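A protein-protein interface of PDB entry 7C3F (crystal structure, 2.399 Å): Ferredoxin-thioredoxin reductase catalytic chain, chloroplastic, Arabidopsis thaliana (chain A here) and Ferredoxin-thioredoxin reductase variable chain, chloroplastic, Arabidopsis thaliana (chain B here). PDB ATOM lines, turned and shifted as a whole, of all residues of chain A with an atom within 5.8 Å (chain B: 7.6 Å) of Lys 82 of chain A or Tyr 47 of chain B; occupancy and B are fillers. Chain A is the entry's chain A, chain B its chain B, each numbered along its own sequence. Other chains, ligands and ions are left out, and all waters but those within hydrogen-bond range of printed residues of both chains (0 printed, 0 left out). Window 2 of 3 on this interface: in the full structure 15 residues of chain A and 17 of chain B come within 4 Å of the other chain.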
ATOM      1  N   SER A  24       5.691 -23.319  -9.997  1.00  0.00           N
ATOM      2  CA  SER A  24       5.790 -22.726 -11.321  1.00  0.00           C
ATOM      3  C   SER A  24       4.443 -22.314 -11.897  1.00  0.00           C
ATOM      4  O   SER A  24       4.413 -21.695 -12.962  1.00  0.00           O
ATOM      5  CB  SER A  24       6.491 -23.694 -12.283  1.00  0.00           C
ATOM      6  OG  SER A  24       6.007 -25.025 -12.139  1.00  0.00           O
ATOM      7  N   GLY A  25       3.342 -22.611 -11.217  1.00  0.00           N
ATOM      8  CA  GLY A  25       2.034 -22.347 -11.793  1.00  0.00           C
ATOM      9  C   GLY A  25       1.731 -23.179 -13.024  1.00  0.00           C
ATOM     10  O   GLY A  25       1.127 -22.674 -13.982  1.00  0.00           O
ATOM     11  N   THR A  26       2.143 -24.444 -13.026  1.00  0.00           N
ATOM     12  CA  THR A  26       1.916 -25.356 -14.137  1.00  0.00           C
ATOM     13  C   THR A  26       1.107 -26.554 -13.663  1.00  0.00           C
ATOM     14  O   THR A  26       0.980 -26.809 -12.462  1.00  0.00           O
ATOM     15  CB  THR A  26       3.239 -25.828 -14.747  1.00  0.00           C
ATOM     16  OG1 THR A  26       4.097 -26.310 -13.705  1.00  0.00           O
ATOM     17  CG2 THR A  26       3.925 -24.683 -15.465  1.00  0.00           C
ATOM     18  N   PRO A  77      15.422 -24.917 -20.188  1.00  0.00           N
ATOM     19  CA  PRO A  77      14.229 -24.377 -20.868  1.00  0.00           C
ATOM     20  C   PRO A  77      12.998 -24.290 -19.981  1.00  0.00           C
ATOM     21  O   PRO A  77      12.188 -23.369 -20.150  1.00  0.00           O
ATOM     22  CB  PRO A  77      14.014 -25.359 -22.027  1.00  0.00           C
ATOM     23  CG  PRO A  77      15.372 -25.868 -22.321  1.00  0.00           C
ATOM     24  CD  PRO A  77      16.035 -26.002 -20.980  1.00  0.00           C
ATOM     25  N   MET A  78      12.830 -25.217 -19.036  1.00  0.00           N
ATOM     26  CA  MET A  78      11.686 -25.136 -18.136  1.00  0.00           C
ATOM     27  C   MET A  78      11.890 -24.056 -17.084  1.00  0.00           C
ATOM     28  O   MET A  78      10.958 -23.310 -16.761  1.00  0.00           O
ATOM     29  CB  MET A  78      11.443 -26.486 -17.469  1.00  0.00           C
ATOM     30  CG  MET A  78      10.334 -26.461 -16.431  1.00  0.00           C
ATOM     31  SD  MET A  78       8.727 -26.106 -17.171  1.00  0.00           S
ATOM     32  CE  MET A  78       7.807 -25.569 -15.728  1.00  0.00           C
ATOM     33  N   ARG A  79      13.100 -23.967 -16.529  1.00  0.00           N
ATOM     34  CA  ARG A  79      13.380 -22.960 -15.512  1.00  0.00           C
ATOM     35  C   ARG A  79      13.277 -21.553 -16.085  1.00  0.00           C
ATOM     36  O   ARG A  79      12.773 -20.640 -15.420  1.00  0.00           O
ATOM     37  CB  ARG A  79      14.763 -23.191 -14.911  1.00  0.00           C
ATOM     38  CG  ARG A  79      14.825 -24.363 -13.957  1.00  0.00           C
ATOM     39  CD  ARG A  79      16.014 -24.231 -13.037  1.00  0.00           C
ATOM     40  NE  ARG A  79      17.253 -24.577 -13.724  1.00  0.00           N
ATOM     41  CZ  ARG A  79      18.097 -25.510 -13.302  1.00  0.00           C
ATOM     42  NH1 ARG A  79      19.205 -25.767 -13.987  1.00  0.00           N
ATOM     43  NH2 ARG A  79      17.834 -26.186 -12.192  1.00  0.00           N
ATOM     44  N   GLU A  80      13.741 -21.359 -17.314  1.00  0.00           N
ATOM     45  CA  GLU A  80      13.795 -20.016 -17.871  1.00  0.00           C
ATOM     46  C   GLU A  80      12.540 -19.664 -18.657  1.00  0.00           C
ATOM     47  O   GLU A  80      12.017 -18.558 -18.506  1.00  0.00           O
ATOM     48  CB  GLU A  80      15.042 -19.864 -18.751  1.00  0.00           C
ATOM     49  CG  GLU A  80      16.349 -19.921 -17.961  1.00  0.00           C
ATOM     50  CD  GLU A  80      17.582 -19.686 -18.819  1.00  0.00           C
ATOM     51  OE1 GLU A  80      17.436 -19.241 -19.976  1.00  0.00           O
ATOM     52  OE2 GLU A  80      18.700 -19.948 -18.332  1.00  0.00           O
ATOM     53  N   ARG A  81      12.025 -20.577 -19.476  1.00  0.00           N
ATOM     54  CA  ARG A  81      10.905 -20.263 -20.354  1.00  0.00           C
ATOM     55  C   ARG A  81       9.629 -21.024 -20.025  1.00  0.00           C
ATOM     56  O   ARG A  81       8.640 -20.878 -20.752  1.00  0.00           O
ATOM     57  CB  ARG A  81      11.296 -20.527 -21.811  1.00  0.00           C
ATOM     58  CG  ARG A  81      12.594 -19.858 -22.211  1.00  0.00           C
ATOM     59  CD  ARG A  81      12.889 -20.024 -23.689  1.00  0.00           C
ATOM     60  NE  ARG A  81      14.247 -19.595 -23.997  1.00  0.00           N
ATOM     61  CZ  ARG A  81      14.671 -19.258 -25.209  1.00  0.00           C
ATOM     62  NH1 ARG A  81      13.837 -19.297 -26.239  1.00  0.00           N
ATOM     63  NH2 ARG A  81      15.929 -18.878 -25.391  1.00  0.00           N
ATOM     64  N   LYS A  82       9.615 -21.821 -18.953  1.00  0.00           N
ATOM     65  CA  LYS A  82       8.466 -22.663 -18.607  1.00  0.00           C
ATOM     66  C   LYS A  82       8.083 -23.597 -19.753  1.00  0.00           C
ATOM     67  O   LYS A  82       6.905 -23.899 -19.952  1.00  0.00           O
ATOM     68  CB  LYS A  82       7.260 -21.820 -18.182  1.00  0.00           C
ATOM     69  CG  LYS A  82       7.270 -21.403 -16.724  1.00  0.00           C
ATOM     70  CD  LYS A  82       6.046 -20.570 -16.387  1.00  0.00           C
ATOM     71  CE  LYS A  82       6.161 -19.947 -15.009  1.00  0.00           C
ATOM     72  NZ  LYS A  82       4.826 -19.802 -14.372  1.00  0.00           N
ATOM     73  N   GLU A  83       9.070 -24.033 -20.529  1.00  0.00           N
ATOM     74  CA  GLU A  83       8.866 -24.969 -21.628  1.00  0.00           C
ATOM     75  C   GLU A  83       9.298 -26.362 -21.184  1.00  0.00           C
ATOM     76  O   GLU A  83      10.475 -26.581 -20.878  1.00  0.00           O
ATOM     77  CB  GLU A  83       9.645 -24.527 -22.866  1.00  0.00           C
ATOM     78  CG  GLU A  83       9.074 -23.284 -23.536  1.00  0.00           C
ATOM     79  CD  GLU A  83       9.950 -22.768 -24.660  1.00  0.00           C
ATOM     80  OE1 GLU A  83       9.688 -21.649 -25.151  1.00  0.00           O
ATOM     81  OE2 GLU A  83      10.901 -23.479 -25.053  1.00  0.00           O
ATOM     82  N   CYS A  84       8.350 -27.295 -21.143  1.00  0.00           N
ATOM     83  CA  CYS A  84       8.617 -28.683 -20.767  1.00  0.00           C
ATOM     84  C   CYS A  84       8.115 -29.577 -21.897  1.00  0.00           C
ATOM     85  O   CYS A  84       6.906 -29.768 -22.055  1.00  0.00           O
ATOM     86  CB  CYS A  84       7.949 -29.010 -19.431  1.00  0.00           C
ATOM     87  SG  CYS A  84       7.685 -30.760 -19.091  1.00  0.00           S
ATOM     88  N   PHE A  89       5.186 -30.641 -17.005  1.00  0.00           N
ATOM     89  CA  PHE A  89       4.701 -29.366 -16.482  1.00  0.00           C
ATOM     90  C   PHE A  89       4.153 -28.561 -17.654  1.00  0.00           C
ATOM     91  O   PHE A  89       4.910 -28.161 -18.544  1.00  0.00           O
ATOM     92  CB  PHE A  89       5.806 -28.588 -15.768  1.00  0.00           C
ATOM     93  CG  PHE A  89       6.565 -29.390 -14.750  1.00  0.00           C
ATOM     94  CD1 PHE A  89       5.973 -29.758 -13.554  1.00  0.00           C
ATOM     95  CD2 PHE A  89       7.880 -29.761 -14.983  1.00  0.00           C
ATOM     96  CE1 PHE A  89       6.669 -30.491 -12.616  1.00  0.00           C
ATOM     97  CE2 PHE A  89       8.583 -30.495 -14.047  1.00  0.00           C
ATOM     98  CZ  PHE A  89       7.976 -30.861 -12.862  1.00  0.00           C
ATOM     99  N   THR A  91       1.724 -25.268 -18.995  1.00  0.00           N
ATOM    100  CA  THR A  91       1.087 -24.005 -18.662  1.00  0.00           C
ATOM    101  C   THR A  91      -0.420 -24.098 -18.904  1.00  0.00           C
ATOM    102  O   THR A  91      -0.872 -24.874 -19.750  1.00  0.00           O
ATOM    103  CB  THR A  91       1.684 -22.867 -19.488  1.00  0.00           C
ATOM    104  OG1 THR A  91       1.463 -23.115 -20.883  1.00  0.00           O
ATOM    105  CG2 THR A  91       3.181 -22.741 -19.229  1.00  0.00           C
ATOM    106  N   LEU B  44      10.185 -12.763 -26.061  1.00  0.00           N
ATOM    107  CA  LEU B  44      10.630 -13.891 -25.248  1.00  0.00           C
ATOM    108  C   LEU B  44      10.513 -13.494 -23.788  1.00  0.00           C
ATOM    109  O   LEU B  44      11.064 -12.465 -23.381  1.00  0.00           O
ATOM    110  CB  LEU B  44      12.069 -14.267 -25.616  1.00  0.00           C
ATOM    111  CG  LEU B  44      12.900 -15.211 -24.753  1.00  0.00           C
ATOM    112  CD1 LEU B  44      12.182 -16.528 -24.531  1.00  0.00           C
ATOM    113  CD2 LEU B  44      14.251 -15.439 -25.418  1.00  0.00           C
ATOM    114  N   LYS B  45       9.803 -14.298 -23.003  1.00  0.00           N
ATOM    115  CA  LYS B  45       9.620 -14.045 -21.582  1.00  0.00           C
ATOM    116  C   LYS B  45      10.328 -15.117 -20.772  1.00  0.00           C
ATOM    117  O   LYS B  45      10.259 -16.305 -21.102  1.00  0.00           O
ATOM    118  CB  LYS B  45       8.133 -14.009 -21.212  1.00  0.00           C
ATOM    119  CG  LYS B  45       7.262 -13.253 -22.203  1.00  0.00           C
ATOM    120  CD  LYS B  45       5.834 -13.110 -21.698  1.00  0.00           C
ATOM    121  CE  LYS B  45       5.027 -12.169 -22.581  1.00  0.00           C
ATOM    122  NZ  LYS B  45       3.562 -12.317 -22.365  1.00  0.00           N
ATOM    123  N   VAL B  46      11.004 -14.691 -19.707  1.00  0.00           N
ATOM    124  CA  VAL B  46      11.732 -15.596 -18.830  1.00  0.00           C
ATOM    125  C   VAL B  46      11.250 -15.389 -17.402  1.00  0.00           C
ATOM    126  O   VAL B  46      10.797 -14.302 -17.031  1.00  0.00           O
ATOM    127  CB  VAL B  46      13.262 -15.408 -18.936  1.00  0.00           C
ATOM    128  CG1 VAL B  46      13.741 -15.761 -20.340  1.00  0.00           C
ATOM    129  CG2 VAL B  46      13.655 -13.986 -18.577  1.00  0.00           C
ATOM    130  N   TYR B  47      11.361 -16.445 -16.593  1.00  0.00           N
ATOM    131  CA  TYR B  47      10.731 -16.493 -15.278  1.00  0.00           C
ATOM    132  C   TYR B  47      11.707 -16.787 -14.146  1.00  0.00           C
ATOM    133  O   TYR B  47      11.272 -17.005 -13.011  1.00  0.00           O
ATOM    134  CB  TYR B  47       9.609 -17.537 -15.269  1.00  0.00           C
ATOM    135  CG  TYR B  47       8.576 -17.338 -16.355  1.00  0.00           C
ATOM    136  CD1 TYR B  47       8.779 -17.839 -17.635  1.00  0.00           C
ATOM    137  CD2 TYR B  47       7.396 -16.651 -16.100  1.00  0.00           C
ATOM    138  CE1 TYR B  47       7.837 -17.658 -18.631  1.00  0.00           C
ATOM    139  CE2 TYR B  47       6.450 -16.465 -17.089  1.00  0.00           C
ATOM    140  CZ  TYR B  47       6.674 -16.970 -18.351  1.00  0.00           C
ATOM    141  OH  TYR B  47       5.732 -16.787 -19.337  1.00  0.00           O
ATOM    142  N   HIS B  48      13.008 -16.800 -14.418  1.00  0.00           N
ATOM    143  CA  HIS B  48      13.998 -17.202 -13.430  1.00  0.00           C
ATOM    144  C   HIS B  48      14.744 -16.031 -12.808  1.00  0.00           C
ATOM    145  O   HIS B  48      15.566 -16.254 -11.913  1.00  0.00           O
ATOM    146  CB  HIS B  48      15.014 -18.164 -14.054  1.00  0.00           C
ATOM    147  CG  HIS B  48      15.771 -17.568 -15.195  1.00  0.00           C
ATOM    148  ND1 HIS B  48      15.147 -17.077 -16.321  1.00  0.00           N
ATOM    149  CD2 HIS B  48      17.097 -17.365 -15.380  1.00  0.00           C
ATOM    150  CE1 HIS B  48      16.056 -16.608 -17.156  1.00  0.00           C
ATOM    151  NE2 HIS B  48      17.248 -16.772 -16.610  1.00  0.00           N
ATOM    152  N   VAL B  49      14.507 -14.801 -13.269  1.00  0.00           N
ATOM    153  CA  VAL B  49      15.197 -13.664 -12.676  1.00  0.00           C
ATOM    154  C   VAL B  49      14.751 -13.539 -11.229  1.00  0.00           C
ATOM    155  O   VAL B  49      13.551 -13.590 -10.925  1.00  0.00           O
ATOM    156  CB  VAL B  49      14.901 -12.384 -13.472  1.00  0.00           C
ATOM    157  CG1 VAL B  49      15.593 -11.186 -12.834  1.00  0.00           C
ATOM    158  CG2 VAL B  49      15.316 -12.554 -14.930  1.00  0.00           C
ATOM    159  N   VAL B  50      15.718 -13.371 -10.326  1.00  0.00           N
ATOM    160  CA  VAL B  50      15.438 -13.514  -8.903  1.00  0.00           C
ATOM    161  C   VAL B  50      14.522 -12.387  -8.443  1.00  0.00           C
ATOM    162  O   VAL B  50      14.805 -11.202  -8.662  1.00  0.00           O
ATOM    163  CB  VAL B  50      16.742 -13.553  -8.091  1.00  0.00           C
ATOM    164  CG1 VAL B  50      17.690 -12.454  -8.533  1.00  0.00           C
ATOM    165  CG2 VAL B  50      16.442 -13.444  -6.605  1.00  0.00           C
ATOM    166  N   ARG B  51      13.411 -12.762  -7.812  1.00  0.00           N
ATOM    167  CA  ARG B  51      12.413 -11.836  -7.280  1.00  0.00           C
ATOM    168  C   ARG B  51      11.838 -10.906  -8.346  1.00  0.00           C
ATOM    169  O   ARG B  51      11.263  -9.864  -8.021  1.00  0.00           O
ATOM    170  CB  ARG B  51      12.975 -11.034  -6.104  1.00  0.00           C
ATOM    171  CG  ARG B  51      13.340 -11.920  -4.923  1.00  0.00           C
ATOM    172  CD  ARG B  51      13.582 -11.126  -3.655  1.00  0.00           C
ATOM    173  NE  ARG B  51      14.981 -10.734  -3.529  1.00  0.00           N
ATOM    174  CZ  ARG B  51      15.488  -9.607  -4.016  1.00  0.00           C
ATOM    175  NH1 ARG B  51      14.709  -8.745  -4.655  1.00  0.00           N
ATOM    176  NH2 ARG B  51      16.776  -9.335  -3.855  1.00  0.00           N
ATOM    177  N   VAL B  52      11.999 -11.257  -9.619  1.00  0.00           N
ATOM    178  CA  VAL B  52      11.257 -10.615 -10.699  1.00  0.00           C
ATOM    179  C   VAL B  52      10.478 -11.733 -11.379  1.00  0.00           C
ATOM    180  O   VAL B  52      11.068 -12.550 -12.101  1.00  0.00           O
ATOM    181  CB  VAL B  52      12.182  -9.882 -11.683  1.00  0.00           C
ATOM    182  CG1 VAL B  52      11.356  -9.124 -12.717  1.00  0.00           C
ATOM    183  CG2 VAL B  52      13.117  -8.941 -10.941  1.00  0.00           C
ATOM    184  N   PRO B  53       9.161 -11.813 -11.178  1.00  0.00           N
ATOM    185  CA  PRO B  53       8.420 -12.993 -11.651  1.00  0.00           C
ATOM    186  C   PRO B  53       8.416 -13.160 -13.158  1.00  0.00           C
ATOM    187  O   PRO B  53       8.296 -14.292 -13.643  1.00  0.00           O
ATOM    188  CB  PRO B  53       7.004 -12.759 -11.103  1.00  0.00           C
ATOM    189  CG  PRO B  53       6.926 -11.286 -10.846  1.00  0.00           C
ATOM    190  CD  PRO B  53       8.303 -10.871 -10.439  1.00  0.00           C
ATOM    191  N   GLU B  54       8.548 -12.078 -13.919  1.00  0.00           N
ATOM    192  CA  GLU B  54       8.461 -12.169 -15.367  1.00  0.00           C
ATOM    193  C   GLU B  54       9.242 -11.023 -15.991  1.00  0.00           C
ATOM    194  O   GLU B  54       9.134  -9.876 -15.551  1.00  0.00           O
ATOM    195  CB  GLU B  54       7.002 -12.145 -15.831  1.00  0.00           C
ATOM    196  CG  GLU B  54       6.812 -12.335 -17.321  1.00  0.00           C
ATOM    197  CD  GLU B  54       5.350 -12.353 -17.716  1.00  0.00           C
ATOM    198  OE1 GLU B  54       5.013 -11.796 -18.781  1.00  0.00           O
ATOM    199  OE2 GLU B  54       4.537 -12.925 -16.957  1.00  0.00           O
ATOM    200  N   VAL B  55      10.023 -11.344 -17.022  1.00  0.00           N
ATOM    201  CA  VAL B  55      10.846 -10.375 -17.733  1.00  0.00           C
ATOM    202  C   VAL B  55      10.679 -10.604 -19.227  1.00  0.00           C
ATOM    203  O   VAL B  55      10.847 -11.728 -19.709  1.00  0.00           O
ATOM    204  CB  VAL B  55      12.337 -10.477 -17.354  1.00  0.00           C
ATOM    205  CG1 VAL B  55      13.155  -9.467 -18.153  1.00  0.00           C
ATOM    206  CG2 VAL B  55      12.536 -10.270 -15.869  1.00  0.00           C
ATOM    207  N   THR B 100      20.505 -15.813 -19.236  1.00  0.00           N
ATOM    208  CA  THR B 100      19.487 -16.562 -19.967  1.00  0.00           C
ATOM    209  C   THR B 100      20.115 -17.178 -21.208  1.00  0.00           C
ATOM    210  O   THR B 100      20.921 -16.536 -21.888  1.00  0.00           O
ATOM    211  CB  THR B 100      18.298 -15.696 -20.423  1.00  0.00           C
ATOM    212  OG1 THR B 100      18.713 -14.850 -21.501  1.00  0.00           O
ATOM    213  CG2 THR B 100      17.758 -14.831 -19.297  1.00  0.00           C
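The side-chain amino group (NZ) of Lys 45 of chain B is in salt-bridge range of the side-chain carboxylate (OE1) of Glu 54 of chain B (3.9 Å). The backbone carbonyl oxygen (O) of Pro 77 of chain A sits at hydrogen-bond distance from the backbone NH (N) of Lys 82 of chain A (3.2 Å). The backbone NH (N) of Val 46 of chain B sits at hydrogen-bond distance from the backbone carbonyl oxygen (O) of Val 55 of chain B (3.0 Å).
The backbone carbonyl oxygen (O) of Glu 80 of chain A lies within hydrogen-bond range of the backbone NH (N) of Tyr 47 of chain B (2.9 Å).
Arg 79 of chain A touches His 48 of chain B (O to CB, 3.6 Å). O of Glu 80 of chain A touches O of Lys 45 of chain B, 3.9 Å away. Val 46 of chain B touches Glu 80 of chain A (CA to O, 3.0 Å). Glu 80 of chain A touches His 48 of chain B (CG to CE1, 3.4 Å). Thr 100 of chain B touches Glu 80 of chain A (CA to OE1, 3.4 Å). Arg 81 of chain A touches Leu 44 of chain B. Arg 81 of chain A touches Tyr 47 of chain B (O to CE1, 3.9 Å). Tyr 47 of chain B touches Lys 82 of chain A.
Of the 13 printed residues of chain A, 4 touch a printed residue of chain B. Printed residues of chain A that touch a printed residue of chain B: Arg 79, Glu 80, Arg 81 and Lys 82. Of the 13 printed residues of chain B, 6 touch a printed residue of chain A. Hydrophobic or aromatic side chains of chain B that line the printed part of chain A: Leu 44, Val 46, Tyr 47 and His 48. Among the printed residues, 9 pairs touch across the chains. Among the printed residues, no Asp or Glu carboxylate lies within 4 Å of a Lys or Arg side-chain nitrogen of the other chain.
Of chain B, only Tyr 47 comes within 4 Å of Lys 82 of chain A. Of the printed residues of chain A, Lys 45 of chain B touches Glu 80. Of the printed residues of chain B, Arg 79 of chain A touches His 48. Printed residues of chain A within 4 Å of Thr 100 of chain B: Glu 80 (3.4 Å). The nearest residue of chain B that does not touch Lys 82 of chain A is Lys 45 of chain B (6.0 Å). The nearest residue of chain A that does not touch Tyr 47 of chain B is Arg 79 of chain A (4.2 Å).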
